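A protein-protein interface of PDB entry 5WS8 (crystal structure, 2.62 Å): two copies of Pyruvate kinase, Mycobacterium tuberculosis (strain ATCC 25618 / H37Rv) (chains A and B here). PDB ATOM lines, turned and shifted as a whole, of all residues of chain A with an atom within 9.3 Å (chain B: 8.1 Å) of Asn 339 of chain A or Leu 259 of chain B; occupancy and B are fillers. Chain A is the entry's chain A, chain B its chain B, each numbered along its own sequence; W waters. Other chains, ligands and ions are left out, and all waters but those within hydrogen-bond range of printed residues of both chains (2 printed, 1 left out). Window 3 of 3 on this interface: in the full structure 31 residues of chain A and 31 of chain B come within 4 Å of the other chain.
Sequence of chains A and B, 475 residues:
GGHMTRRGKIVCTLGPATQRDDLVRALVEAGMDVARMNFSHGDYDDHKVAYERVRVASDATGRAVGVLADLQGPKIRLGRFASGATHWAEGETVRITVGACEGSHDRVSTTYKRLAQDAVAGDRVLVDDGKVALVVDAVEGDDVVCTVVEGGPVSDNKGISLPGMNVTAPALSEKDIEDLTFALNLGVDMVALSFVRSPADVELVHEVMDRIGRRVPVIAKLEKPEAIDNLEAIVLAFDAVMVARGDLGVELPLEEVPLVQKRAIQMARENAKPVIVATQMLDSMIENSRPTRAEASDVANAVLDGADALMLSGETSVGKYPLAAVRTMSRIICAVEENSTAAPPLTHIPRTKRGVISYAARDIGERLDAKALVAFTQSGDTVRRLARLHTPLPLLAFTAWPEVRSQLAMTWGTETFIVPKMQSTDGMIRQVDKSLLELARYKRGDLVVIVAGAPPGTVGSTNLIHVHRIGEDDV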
ATOM      1  N   ARG A 293      21.899  19.053  -1.078  1.00  0.00           N
ATOM      2  CA  ARG A 293      23.080  18.259  -0.946  1.00  0.00           C
ATOM      3  C   ARG A 293      22.869  17.154   0.085  1.00  0.00           C
ATOM      4  O   ARG A 293      23.447  16.074  -0.032  1.00  0.00           O
ATOM      5  CB  ARG A 293      24.260  19.138  -0.574  1.00  0.00           C
ATOM      6  CG  ARG A 293      24.551  20.250  -1.569  1.00  0.00           C
ATOM      7  CD  ARG A 293      25.015  19.718  -2.917  1.00  0.00           C
ATOM      8  NE  ARG A 293      25.167  20.828  -3.820  1.00  0.00           N
ATOM      9  CZ  ARG A 293      24.175  21.365  -4.504  1.00  0.00           C
ATOM     10  NH1 ARG A 293      22.946  20.853  -4.449  1.00  0.00           N
ATOM     11  NH2 ARG A 293      24.416  22.412  -5.253  1.00  0.00           N
ATOM     12  N   ALA A 296      20.759  14.332  -1.781  1.00  0.00           N
ATOM     13  CA  ALA A 296      21.620  13.492  -2.629  1.00  0.00           C
ATOM     14  C   ALA A 296      22.464  12.538  -1.763  1.00  0.00           C
ATOM     15  O   ALA A 296      22.623  11.372  -2.089  1.00  0.00           O
ATOM     16  CB  ALA A 296      22.522  14.350  -3.510  1.00  0.00           C
ATOM     17  N   SER A 297      22.990  13.048  -0.662  1.00  0.00           N
ATOM     18  CA  SER A 297      23.825  12.262   0.236  1.00  0.00           C
ATOM     19  C   SER A 297      23.037  11.142   0.894  1.00  0.00           C
ATOM     20  O   SER A 297      23.549  10.038   1.099  1.00  0.00           O
ATOM     21  CB  SER A 297      24.429  13.159   1.322  1.00  0.00           C
ATOM     22  OG  SER A 297      25.216  12.405   2.203  1.00  0.00           O
ATOM     23  N   ALA A 300      22.473   8.359  -1.687  1.00  0.00           N
ATOM     24  CA  ALA A 300      23.745   7.661  -1.893  1.00  0.00           C
ATOM     25  C   ALA A 300      24.066   6.774  -0.711  1.00  0.00           C
ATOM     26  O   ALA A 300      24.506   5.654  -0.888  1.00  0.00           O
ATOM     27  CB  ALA A 300      24.890   8.642  -2.119  1.00  0.00           C
ATOM     28  N   ASN A 301      23.821   7.273   0.494  1.00  0.00           N
ATOM     29  CA  ASN A 301      24.135   6.526   1.685  1.00  0.00           C
ATOM     30  C   ASN A 301      23.228   5.341   1.914  1.00  0.00           C
ATOM     31  O   ASN A 301      23.688   4.306   2.368  1.00  0.00           O
ATOM     32  CB  ASN A 301      24.220   7.439   2.920  1.00  0.00           C
ATOM     33  CG  ASN A 301      25.610   8.046   3.071  1.00  0.00           C
ATOM     34  OD1 ASN A 301      26.575   7.313   3.337  1.00  0.00           O
ATOM     35  ND2 ASN A 301      25.742   9.363   2.836  1.00  0.00           N
ATOM     36  N   VAL A 303      22.094   3.526  -0.513  1.00  0.00           N
ATOM     37  CA  VAL A 303      22.596   2.514  -1.427  1.00  0.00           C
ATOM     38  C   VAL A 303      23.808   1.773  -0.852  1.00  0.00           C
ATOM     39  O   VAL A 303      23.912   0.548  -0.992  1.00  0.00           O
ATOM     40  CB  VAL A 303      22.958   3.126  -2.780  1.00  0.00           C
ATOM     41  CG1 VAL A 303      23.827   2.162  -3.597  1.00  0.00           C
ATOM     42  CG2 VAL A 303      21.687   3.525  -3.525  1.00  0.00           C
ATOM     43  N   LEU A 304      24.728   2.532  -0.248  1.00  0.00           N
ATOM     44  CA  LEU A 304      25.904   1.991   0.385  1.00  0.00           C
ATOM     45  C   LEU A 304      25.563   1.216   1.654  1.00  0.00           C
ATOM     46  O   LEU A 304      26.265   0.285   2.025  1.00  0.00           O
ATOM     47  CB  LEU A 304      26.872   3.110   0.746  1.00  0.00           C
ATOM     48  CG  LEU A 304      27.502   3.864  -0.419  1.00  0.00           C
ATOM     49  CD1 LEU A 304      28.107   5.197   0.020  1.00  0.00           C
ATOM     50  CD2 LEU A 304      28.556   2.994  -1.081  1.00  0.00           C
ATOM     51  N   ARG A 331      19.746   8.527 -11.156  1.00  0.00           N
ATOM     52  CA  ARG A 331      21.110   8.962 -11.417  1.00  0.00           C
ATOM     53  C   ARG A 331      22.018   8.805 -10.205  1.00  0.00           C
ATOM     54  O   ARG A 331      23.165   8.424 -10.338  1.00  0.00           O
ATOM     55  CB  ARG A 331      21.129  10.409 -11.851  1.00  0.00           C
ATOM     56  CG  ARG A 331      20.608  10.628 -13.246  1.00  0.00           C
ATOM     57  CD  ARG A 331      21.074  11.967 -13.814  1.00  0.00           C
ATOM     58  NE  ARG A 331      20.301  13.072 -13.273  1.00  0.00           N
ATOM     59  CZ  ARG A 331      19.070  13.383 -13.669  1.00  0.00           C
ATOM     60  NH1 ARG A 331      18.473  12.692 -14.642  1.00  0.00           N
ATOM     61  NH2 ARG A 331      18.435  14.396 -13.102  1.00  0.00           N
ATOM     62  N   ILE A 332      21.520   9.140  -9.024  1.00  0.00           N
ATOM     63  CA  ILE A 332      22.351   9.067  -7.825  1.00  0.00           C
ATOM     64  C   ILE A 332      22.698   7.612  -7.556  1.00  0.00           C
ATOM     65  O   ILE A 332      23.852   7.272  -7.327  1.00  0.00           O
ATOM     66  CB  ILE A 332      21.653   9.677  -6.599  1.00  0.00           C
ATOM     67  CG1 ILE A 332      21.532  11.182  -6.753  1.00  0.00           C
ATOM     68  CG2 ILE A 332      22.449   9.382  -5.351  1.00  0.00           C
ATOM     69  CD1 ILE A 332      20.382  11.769  -5.979  1.00  0.00           C
ATOM     70  N   ILE A 333      21.696   6.751  -7.619  1.00  0.00           N
ATOM     71  CA  ILE A 333      21.906   5.334  -7.417  1.00  0.00           C
ATOM     72  C   ILE A 333      22.970   4.817  -8.387  1.00  0.00           C
ATOM     73  O   ILE A 333      23.940   4.158  -7.973  1.00  0.00           O
ATOM     74  CB  ILE A 333      20.602   4.550  -7.615  1.00  0.00           C
ATOM     75  CG1 ILE A 333      19.622   4.906  -6.506  1.00  0.00           C
ATOM     76  CG2 ILE A 333      20.876   3.052  -7.581  1.00  0.00           C
ATOM     77  CD1 ILE A 333      18.299   4.202  -6.599  1.00  0.00           C
ATOM     78  N   CYS A 334      22.800   5.138  -9.667  1.00  0.00           N
ATOM     79  CA  CYS A 334      23.735   4.701 -10.672  1.00  0.00           C
ATOM     80  C   CYS A 334      25.126   5.277 -10.405  1.00  0.00           C
ATOM     81  O   CYS A 334      26.110   4.580 -10.558  1.00  0.00           O
ATOM     82  CB  CYS A 334      23.246   5.054 -12.090  1.00  0.00           C
ATOM     83  SG  CYS A 334      21.935   3.971 -12.723  1.00  0.00           S
ATOM     84  N   ALA A 335      25.218   6.537  -9.999  1.00  0.00           N
ATOM     85  CA  ALA A 335      26.533   7.153  -9.772  1.00  0.00           C
ATOM     86  C   ALA A 335      27.264   6.400  -8.722  1.00  0.00           C
ATOM     87  O   ALA A 335      28.454   6.140  -8.870  1.00  0.00           O
ATOM     88  CB  ALA A 335      26.406   8.601  -9.359  1.00  0.00           C
ATOM     89  N   VAL A 336      26.556   6.022  -7.666  1.00  0.00           N
ATOM     90  CA  VAL A 336      27.176   5.261  -6.596  1.00  0.00           C
ATOM     91  C   VAL A 336      27.593   3.882  -7.051  1.00  0.00           C
ATOM     92  O   VAL A 336      28.727   3.475  -6.825  1.00  0.00           O
ATOM     93  CB  VAL A 336      26.235   5.115  -5.404  1.00  0.00           C
ATOM     94  CG1 VAL A 336      26.859   4.242  -4.327  1.00  0.00           C
ATOM     95  CG2 VAL A 336      25.930   6.480  -4.849  1.00  0.00           C
ATOM     96  N   GLU A 337      26.669   3.164  -7.693  1.00  0.00           N
ATOM     97  CA  GLU A 337      26.939   1.785  -8.166  1.00  0.00           C
ATOM     98  C   GLU A 337      28.049   1.664  -9.211  1.00  0.00           C
ATOM     99  O   GLU A 337      28.751   0.668  -9.242  1.00  0.00           O
ATOM    100  CB  GLU A 337      25.677   1.150  -8.715  1.00  0.00           C
ATOM    101  CG  GLU A 337      24.654   0.765  -7.658  1.00  0.00           C
ATOM    102  CD  GLU A 337      23.272   0.494  -8.256  1.00  0.00           C
ATOM    103  OE1 GLU A 337      23.124   0.535  -9.513  1.00  0.00           O
ATOM    104  OE2 GLU A 337      22.329   0.239  -7.461  1.00  0.00           O
ATOM    105  N   GLU A 338      28.202   2.659 -10.071  1.00  0.00           N
ATOM    106  CA  GLU A 338      29.236   2.608 -11.092  1.00  0.00           C
ATOM    107  C   GLU A 338      30.601   2.549 -10.424  1.00  0.00           C
ATOM    108  O   GLU A 338      31.515   1.838 -10.863  1.00  0.00           O
ATOM    109  CB  GLU A 338      29.134   3.817 -11.993  1.00  0.00           C
ATOM    110  CG  GLU A 338      30.393   4.077 -12.781  1.00  0.00           C
ATOM    111  CD  GLU A 338      30.182   5.022 -13.955  1.00  0.00           C
ATOM    112  OE1 GLU A 338      31.183   5.257 -14.698  1.00  0.00           O
ATOM    113  OE2 GLU A 338      29.026   5.519 -14.141  1.00  0.00           O
ATOM    114  N   ASN A 339      30.743   3.310  -9.353  1.00  0.00           N
ATOM    115  CA  ASN A 339      31.958   3.283  -8.612  1.00  0.00           C
ATOM    116  C   ASN A 339      32.142   1.892  -8.023  1.00  0.00           C
ATOM    117  O   ASN A 339      33.105   1.203  -8.351  1.00  0.00           O
ATOM    118  CB  ASN A 339      31.954   4.316  -7.514  1.00  0.00           C
ATOM    119  CG  ASN A 339      33.066   4.078  -6.539  1.00  0.00           C
ATOM    120  OD1 ASN A 339      32.852   3.542  -5.449  1.00  0.00           O
ATOM    121  ND2 ASN A 339      34.285   4.371  -6.968  1.00  0.00           N
ATOM    122  N   SER A 340      31.199   1.467  -7.181  1.00  0.00           N
ATOM    123  CA  SER A 340      31.238   0.116  -6.606  1.00  0.00           C
ATOM    124  C   SER A 340      29.869  -0.355  -6.178  1.00  0.00           C
ATOM    125  O   SER A 340      29.025   0.446  -5.797  1.00  0.00           O
ATOM    126  CB  SER A 340      32.173   0.086  -5.403  1.00  0.00           C
ATOM    127  OG  SER A 340      31.861  -0.991  -4.541  1.00  0.00           O
ATOM    128  N   THR A 341      29.650  -1.661  -6.210  1.00  0.00           N
ATOM    129  CA  THR A 341      28.369  -2.203  -5.746  1.00  0.00           C
ATOM    130  C   THR A 341      28.526  -2.855  -4.363  1.00  0.00           C
ATOM    131  O   THR A 341      27.571  -3.460  -3.845  1.00  0.00           O
ATOM    132  CB  THR A 341      27.755  -3.230  -6.745  1.00  0.00           C
ATOM    133  OG1 THR A 341      28.504  -4.468  -6.717  1.00  0.00           O
ATOM    134  CG2 THR A 341      27.716  -2.655  -8.174  1.00  0.00           C
ATOM    135  N   ALA A 342      29.714  -2.698  -3.764  1.00  0.00           N
ATOM    136  CA  ALA A 342      30.032  -3.277  -2.448  1.00  0.00           C
ATOM    137  C   ALA A 342      29.147  -2.770  -1.334  1.00  0.00           C
ATOM    138  O   ALA A 342      28.983  -1.558  -1.145  1.00  0.00           O
ATOM    139  CB  ALA A 342      31.482  -3.016  -2.078  1.00  0.00           C
ATOM    140  N   PRO A 392      28.469  -7.739  -8.484  1.00  0.00           N
ATOM    141  CA  PRO A 392      28.374  -6.888  -9.688  1.00  0.00           C
ATOM    142  C   PRO A 392      27.896  -7.640 -10.929  1.00  0.00           C
ATOM    143  O   PRO A 392      27.622  -7.023 -11.964  1.00  0.00           O
ATOM    144  CB  PRO A 392      29.813  -6.393  -9.901  1.00  0.00           C
ATOM    145  CG  PRO A 392      30.674  -7.362  -9.170  1.00  0.00           C
ATOM    146  CD  PRO A 392      29.860  -7.931  -8.040  1.00  0.00           C
ATOM    147  N   ILE B 228      39.306  18.645  -7.560  1.00  0.00           N
ATOM    148  CA  ILE B 228      39.143  17.222  -7.299  1.00  0.00           C
ATOM    149  C   ILE B 228      40.158  16.383  -8.088  1.00  0.00           C
ATOM    150  O   ILE B 228      40.549  15.303  -7.646  1.00  0.00           O
ATOM    151  CB  ILE B 228      37.709  16.762  -7.600  1.00  0.00           C
ATOM    152  CG1 ILE B 228      36.703  17.543  -6.733  1.00  0.00           C
ATOM    153  CG2 ILE B 228      37.568  15.273  -7.366  1.00  0.00           C
ATOM    154  CD1 ILE B 228      37.073  17.643  -5.265  1.00  0.00           C
ATOM    155  N   LEU B 231      43.251  16.674  -5.980  1.00  0.00           N
ATOM    156  CA  LEU B 231      42.897  16.556  -4.574  1.00  0.00           C
ATOM    157  C   LEU B 231      44.110  16.259  -3.685  1.00  0.00           C
ATOM    158  O   LEU B 231      44.297  16.902  -2.675  1.00  0.00           O
ATOM    159  CB  LEU B 231      41.831  15.479  -4.385  1.00  0.00           C
ATOM    160  CG  LEU B 231      41.312  15.225  -2.979  1.00  0.00           C
ATOM    161  CD1 LEU B 231      40.567  16.428  -2.455  1.00  0.00           C
ATOM    162  CD2 LEU B 231      40.400  14.010  -2.989  1.00  0.00           C
ATOM    163  N   VAL B 243      34.892  20.474   2.201  1.00  0.00           N
ATOM    164  CA  VAL B 243      34.099  19.991   1.103  1.00  0.00           C
ATOM    165  C   VAL B 243      32.938  20.954   0.934  1.00  0.00           C
ATOM    166  O   VAL B 243      31.980  20.926   1.687  1.00  0.00           O
ATOM    167  CB  VAL B 243      33.577  18.580   1.376  1.00  0.00           C
ATOM    168  CG1 VAL B 243      32.738  18.100   0.208  1.00  0.00           C
ATOM    169  CG2 VAL B 243      34.730  17.623   1.573  1.00  0.00           C
ATOM    170  N   LEU B 248      30.034  22.807  -5.197  1.00  0.00           N
ATOM    171  CA  LEU B 248      30.526  21.548  -5.742  1.00  0.00           C
ATOM    172  C   LEU B 248      29.421  20.833  -6.522  1.00  0.00           C
ATOM    173  O   LEU B 248      29.682  20.194  -7.536  1.00  0.00           O
ATOM    174  CB  LEU B 248      31.102  20.653  -4.643  1.00  0.00           C
ATOM    175  CG  LEU B 248      31.983  19.481  -5.096  1.00  0.00           C
ATOM    176  CD1 LEU B 248      33.222  19.926  -5.869  1.00  0.00           C
ATOM    177  CD2 LEU B 248      32.413  18.655  -3.902  1.00  0.00           C
ATOM    178  N   LEU B 254      25.511  16.821  -9.396  1.00  0.00           N
ATOM    179  CA  LEU B 254      25.216  16.675  -7.971  1.00  0.00           C
ATOM    180  C   LEU B 254      25.241  15.216  -7.523  1.00  0.00           C
ATOM    181  O   LEU B 254      25.467  14.928  -6.355  1.00  0.00           O
ATOM    182  CB  LEU B 254      23.884  17.338  -7.601  1.00  0.00           C
ATOM    183  CG  LEU B 254      22.621  16.786  -8.262  1.00  0.00           C
ATOM    184  CD1 LEU B 254      22.080  15.614  -7.448  1.00  0.00           C
ATOM    185  CD2 LEU B 254      21.572  17.888  -8.407  1.00  0.00           C
ATOM    186  N   GLU B 255      25.029  14.301  -8.455  1.00  0.00           N
ATOM    187  CA  GLU B 255      25.033  12.890  -8.129  1.00  0.00           C
ATOM    188  C   GLU B 255      26.441  12.350  -7.775  1.00  0.00           C
ATOM    189  O   GLU B 255      26.565  11.280  -7.197  1.00  0.00           O
ATOM    190  CB  GLU B 255      24.391  12.068  -9.272  1.00  0.00           C
ATOM    191  CG  GLU B 255      24.966  12.306 -10.660  1.00  0.00           C
ATOM    192  CD  GLU B 255      24.229  13.397 -11.441  1.00  0.00           C
ATOM    193  OE1 GLU B 255      23.821  14.407 -10.831  1.00  0.00           O
ATOM    194  OE2 GLU B 255      24.077  13.263 -12.682  1.00  0.00           O
ATOM    195  N   GLU B 256      27.485  13.095  -8.125  1.00  0.00           N
ATOM    196  CA  GLU B 256      28.861  12.681  -7.877  1.00  0.00           C
ATOM    197  C   GLU B 256      29.385  13.216  -6.552  1.00  0.00           C
ATOM    198  O   GLU B 256      30.447  12.808  -6.073  1.00  0.00           O
ATOM    199  CB  GLU B 256      29.765  13.174  -9.004  1.00  0.00           C
ATOM    200  CG  GLU B 256      29.376  12.629 -10.371  1.00  0.00           C
ATOM    201  CD  GLU B 256      30.303  13.080 -11.505  1.00  0.00           C
ATOM    202  OE1 GLU B 256      31.217  13.922 -11.277  1.00  0.00           O
ATOM    203  OE2 GLU B 256      30.120  12.571 -12.634  1.00  0.00           O
ATOM    204  N   VAL B 257      28.656  14.140  -5.960  1.00  0.00           N
ATOM    205  CA  VAL B 257      29.178  14.857  -4.819  1.00  0.00           C
ATOM    206  C   VAL B 257      29.378  13.935  -3.627  1.00  0.00           C
ATOM    207  O   VAL B 257      30.354  14.068  -2.909  1.00  0.00           O
ATOM    208  CB  VAL B 257      28.279  16.058  -4.452  1.00  0.00           C
ATOM    209  CG1 VAL B 257      28.656  16.636  -3.106  1.00  0.00           C
ATOM    210  CG2 VAL B 257      28.401  17.124  -5.518  1.00  0.00           C
ATOM    211  N   PRO B 258      28.442  13.014  -3.391  1.00  0.00           N
ATOM    212  CA  PRO B 258      28.581  12.150  -2.223  1.00  0.00           C
ATOM    213  C   PRO B 258      29.842  11.280  -2.195  1.00  0.00           C
ATOM    214  O   PRO B 258      30.352  11.004  -1.142  1.00  0.00           O
ATOM    215  CB  PRO B 258      27.326  11.279  -2.289  1.00  0.00           C
ATOM    216  CG  PRO B 258      26.318  12.164  -2.908  1.00  0.00           C
ATOM    217  CD  PRO B 258      27.087  12.929  -3.966  1.00  0.00           C
ATOM    218  N   LEU B 259      30.324  10.828  -3.332  1.00  0.00           N
ATOM    219  CA  LEU B 259      31.520  10.027  -3.335  1.00  0.00           C
ATOM    220  C   LEU B 259      32.753  10.891  -3.291  1.00  0.00           C
ATOM    221  O   LEU B 259      33.786  10.477  -2.783  1.00  0.00           O
ATOM    222  CB  LEU B 259      31.569   9.159  -4.561  1.00  0.00           C
ATOM    223  CG  LEU B 259      30.593   7.996  -4.554  1.00  0.00           C
ATOM    224  CD1 LEU B 259      30.935   7.039  -5.701  1.00  0.00           C
ATOM    225  CD2 LEU B 259      30.584   7.257  -3.215  1.00  0.00           C
ATOM    226  N   VAL B 260      32.666  12.084  -3.862  1.00  0.00           N
ATOM    227  CA  VAL B 260      33.764  13.006  -3.779  1.00  0.00           C
ATOM    228  C   VAL B 260      33.958  13.370  -2.330  1.00  0.00           C
ATOM    229  O   VAL B 260      35.071  13.394  -1.846  1.00  0.00           O
ATOM    230  CB  VAL B 260      33.507  14.261  -4.609  1.00  0.00           C
ATOM    231  CG1 VAL B 260      34.497  15.343  -4.242  1.00  0.00           C
ATOM    232  CG2 VAL B 260      33.614  13.928  -6.088  1.00  0.00           C
ATOM    233  N   GLN B 261      32.864  13.626  -1.623  1.00  0.00           N
ATOM    234  CA  GLN B 261      32.946  13.926  -0.195  1.00  0.00           C
ATOM    235  C   GLN B 261      33.714  12.831   0.566  1.00  0.00           C
ATOM    236  O   GLN B 261      34.573  13.131   1.367  1.00  0.00           O
ATOM    237  CB  GLN B 261      31.544  14.128   0.408  1.00  0.00           C
ATOM    238  CG  GLN B 261      31.507  14.100   1.929  1.00  0.00           C
ATOM    239  CD  GLN B 261      30.133  14.426   2.515  1.00  0.00           C
ATOM    240  OE1 GLN B 261      29.459  15.323   2.054  1.00  0.00           O
ATOM    241  NE2 GLN B 261      29.732  13.695   3.547  1.00  0.00           N
ATOM    242  N   LYS B 262      33.412  11.566   0.318  1.00  0.00           N
ATOM    243  CA  LYS B 262      34.040  10.495   1.085  1.00  0.00           C
ATOM    244  C   LYS B 262      35.481  10.345   0.741  1.00  0.00           C
ATOM    245  O   LYS B 262      36.291  10.031   1.583  1.00  0.00           O
ATOM    246  CB  LYS B 262      33.300   9.190   0.889  1.00  0.00           C
ATOM    247  CG  LYS B 262      31.881   9.274   1.425  1.00  0.00           C
ATOM    248  CD  LYS B 262      30.981   8.201   0.858  1.00  0.00           C
ATOM    249  CE  LYS B 262      29.542   8.428   1.318  1.00  0.00           C
ATOM    250  NZ  LYS B 262      29.250   7.947   2.696  1.00  0.00           N
ATOM    251  N   ARG B 263      35.802  10.633  -0.499  1.00  0.00           N
ATOM    252  CA  ARG B 263      37.151  10.490  -0.998  1.00  0.00           C
ATOM    253  C   ARG B 263      38.058  11.561  -0.413  1.00  0.00           C
ATOM    254  O   ARG B 263      39.230  11.322  -0.168  1.00  0.00           O
ATOM    255  CB  ARG B 263      37.144  10.635  -2.498  1.00  0.00           C
ATOM    256  CG  ARG B 263      37.517   9.399  -3.264  1.00  0.00           C
ATOM    257  CD  ARG B 263      37.605   9.735  -4.752  1.00  0.00           C
ATOM    258  NE  ARG B 263      38.894  10.368  -5.102  1.00  0.00           N
ATOM    259  CZ  ARG B 263      39.061  11.293  -6.053  1.00  0.00           C
ATOM    260  NH1 ARG B 263      38.011  11.745  -6.749  1.00  0.00           N
ATOM    261  NH2 ARG B 263      40.283  11.788  -6.289  1.00  0.00           N
ATOM    262  N   ALA B 264      37.506  12.754  -0.238  1.00  0.00           N
ATOM    263  CA  ALA B 264      38.238  13.902   0.291  1.00  0.00           C
ATOM    264  C   ALA B 264      38.488  13.764   1.782  1.00  0.00           C
ATOM    265  O   ALA B 264      39.563  14.087   2.262  1.00  0.00           O
ATOM    266  CB  ALA B 264      37.459  15.188   0.029  1.00  0.00           C
ATOM    267  N   ILE B 265      37.481  13.310   2.516  1.00  0.00           N
ATOM    268  CA  ILE B 265      37.631  13.073   3.947  1.00  0.00           C
ATOM    269  C   ILE B 265      38.721  12.033   4.183  1.00  0.00           C
ATOM    270  O   ILE B 265      39.571  12.210   5.031  1.00  0.00           O
ATOM    271  CB  ILE B 265      36.310  12.592   4.563  1.00  0.00           C
ATOM    272  CG1 ILE B 265      35.294  13.740   4.603  1.00  0.00           C
ATOM    273  CG2 ILE B 265      36.527  12.006   5.949  1.00  0.00           C
ATOM    274  CD1 ILE B 265      33.855  13.273   4.703  1.00  0.00           C
ATOM    275  N   GLN B 266      38.703  10.954   3.410  1.00  0.00           N
ATOM    276  CA  GLN B 266      39.698   9.887   3.545  1.00  0.00           C
ATOM    277  C   GLN B 266      41.094  10.440   3.226  1.00  0.00           C
ATOM    278  O   GLN B 266      42.057  10.128   3.900  1.00  0.00           O
ATOM    279  CB  GLN B 266      39.358   8.710   2.606  1.00  0.00           C
ATOM    280  CG  GLN B 266      40.234   7.489   2.794  1.00  0.00           C
ATOM    281  CD  GLN B 266      39.900   6.689   4.049  1.00  0.00           C
ATOM    282  OE1 GLN B 266      38.812   6.816   4.623  1.00  0.00           O
ATOM    283  NE2 GLN B 266      40.839   5.826   4.465  1.00  0.00           N
ATOM    284  N   ASP B 305      31.683   8.965   7.932  1.00  0.00           N
ATOM    285  CA  ASP B 305      32.709   9.130   6.898  1.00  0.00           C
ATOM    286  C   ASP B 305      34.063   9.431   7.563  1.00  0.00           C
ATOM    287  O   ASP B 305      35.109   9.085   7.039  1.00  0.00           O
ATOM    288  CB  ASP B 305      32.349  10.286   5.932  1.00  0.00           C
ATOM    289  CG  ASP B 305      31.097   9.991   5.052  1.00  0.00           C
ATOM    290  OD1 ASP B 305      30.624   8.825   5.053  1.00  0.00           O
ATOM    291  OD2 ASP B 305      30.594  10.936   4.358  1.00  0.00           O
HETATM  292  O   HOH W   1      27.972  11.846   1.422  1.00  0.00           O
HETATM  293  O   HOH W   2      26.968  13.376   4.530  1.00  0.00           O
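NZ of Lys 262 of chain B lies within hydrogen-bond range of OD1 of Asn 301 of chain A, 2.8 Å away.
The side-chain carboxylate (OE2) of Glu 255 of chain B lies within salt-bridge range of the guanidinium group (NE) of Arg 331 of chain A, at 3.8 Å.
O of Ser 297 of chain A is in hydrogen-bond range of ND2 of Asn 301 of chain A, at 2.9 Å.
The side-chain amino group (NZ) of Lys 262 of chain B is in salt-bridge range of the side-chain carboxylate (OD1) of Asp 305 of chain B (2.9 Å).
Among the printed residues, pairs that only touch across the chains: Ala 296 of chain A with Pro 258 of chain B (3.9 Å), Ala 300 of chain A with Pro 258 of chain B (3.6 Å), Leu 304 of chain A with Lys 262 of chain B (3.8 Å), Ile 332 of chain A with Glu 255 of chain B (3.9 Å), Ala 335 of chain A with Glu 255 of chain B (3.4 Å) and Asn 339 of chain A with Leu 259 of chain B (3.4 Å).
Printed residues of chain B within 4 Å of Ala 296 of chain A: Pro 258 (3.9 Å).
Of the printed residues of chain B, Asn 301 of chain A touches Lys 262 (2.8 Å).
Printed residues of chain B within 4 Å of Leu 304 of chain A: Lys 262.
Ile 333 of chain A touches none of the printed residues of chain B.
Asn 339 of chain A touches just one residue of chain B: Leu 259.
Leu 259 of chain B touches just one residue of chain A: Asn 339.
No residue of chain A comes within 4 Å of Val 260 of chain B.
The nearest residue of chain A that does not touch Leu 259 of chain B is Ala 335 of chain A (4.1 Å).
The nearest printed residue of chain B that does not touch Arg 331 of chain A is Leu 254 of chain B (6.6 Å).
Printed residues of chain B that touch a printed residue of chain A: Glu 255, Pro 258, Leu 259 and Lys 262.
Of the 20 printed residues of chain A, 8 touch a printed residue of chain B.
Among the printed residues, Asp or Glu carboxylates within 4 Å of a Lys or Arg side-chain nitrogen of the other chain: Arg 331 of chain A with Glu 255 of chain B.
No position is printed for both chains.
Water W1 lies within hydrogen-bond range of OG of Ser 297 of chain A (2.9 Å) and NE2 of Gln 261 of chain B (3.3 Å).
Water W2 bridges the side-chain amide nitrogen of Gln 261 of chain B and the side-chain hydroxyl of Ser 297 of chain A.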
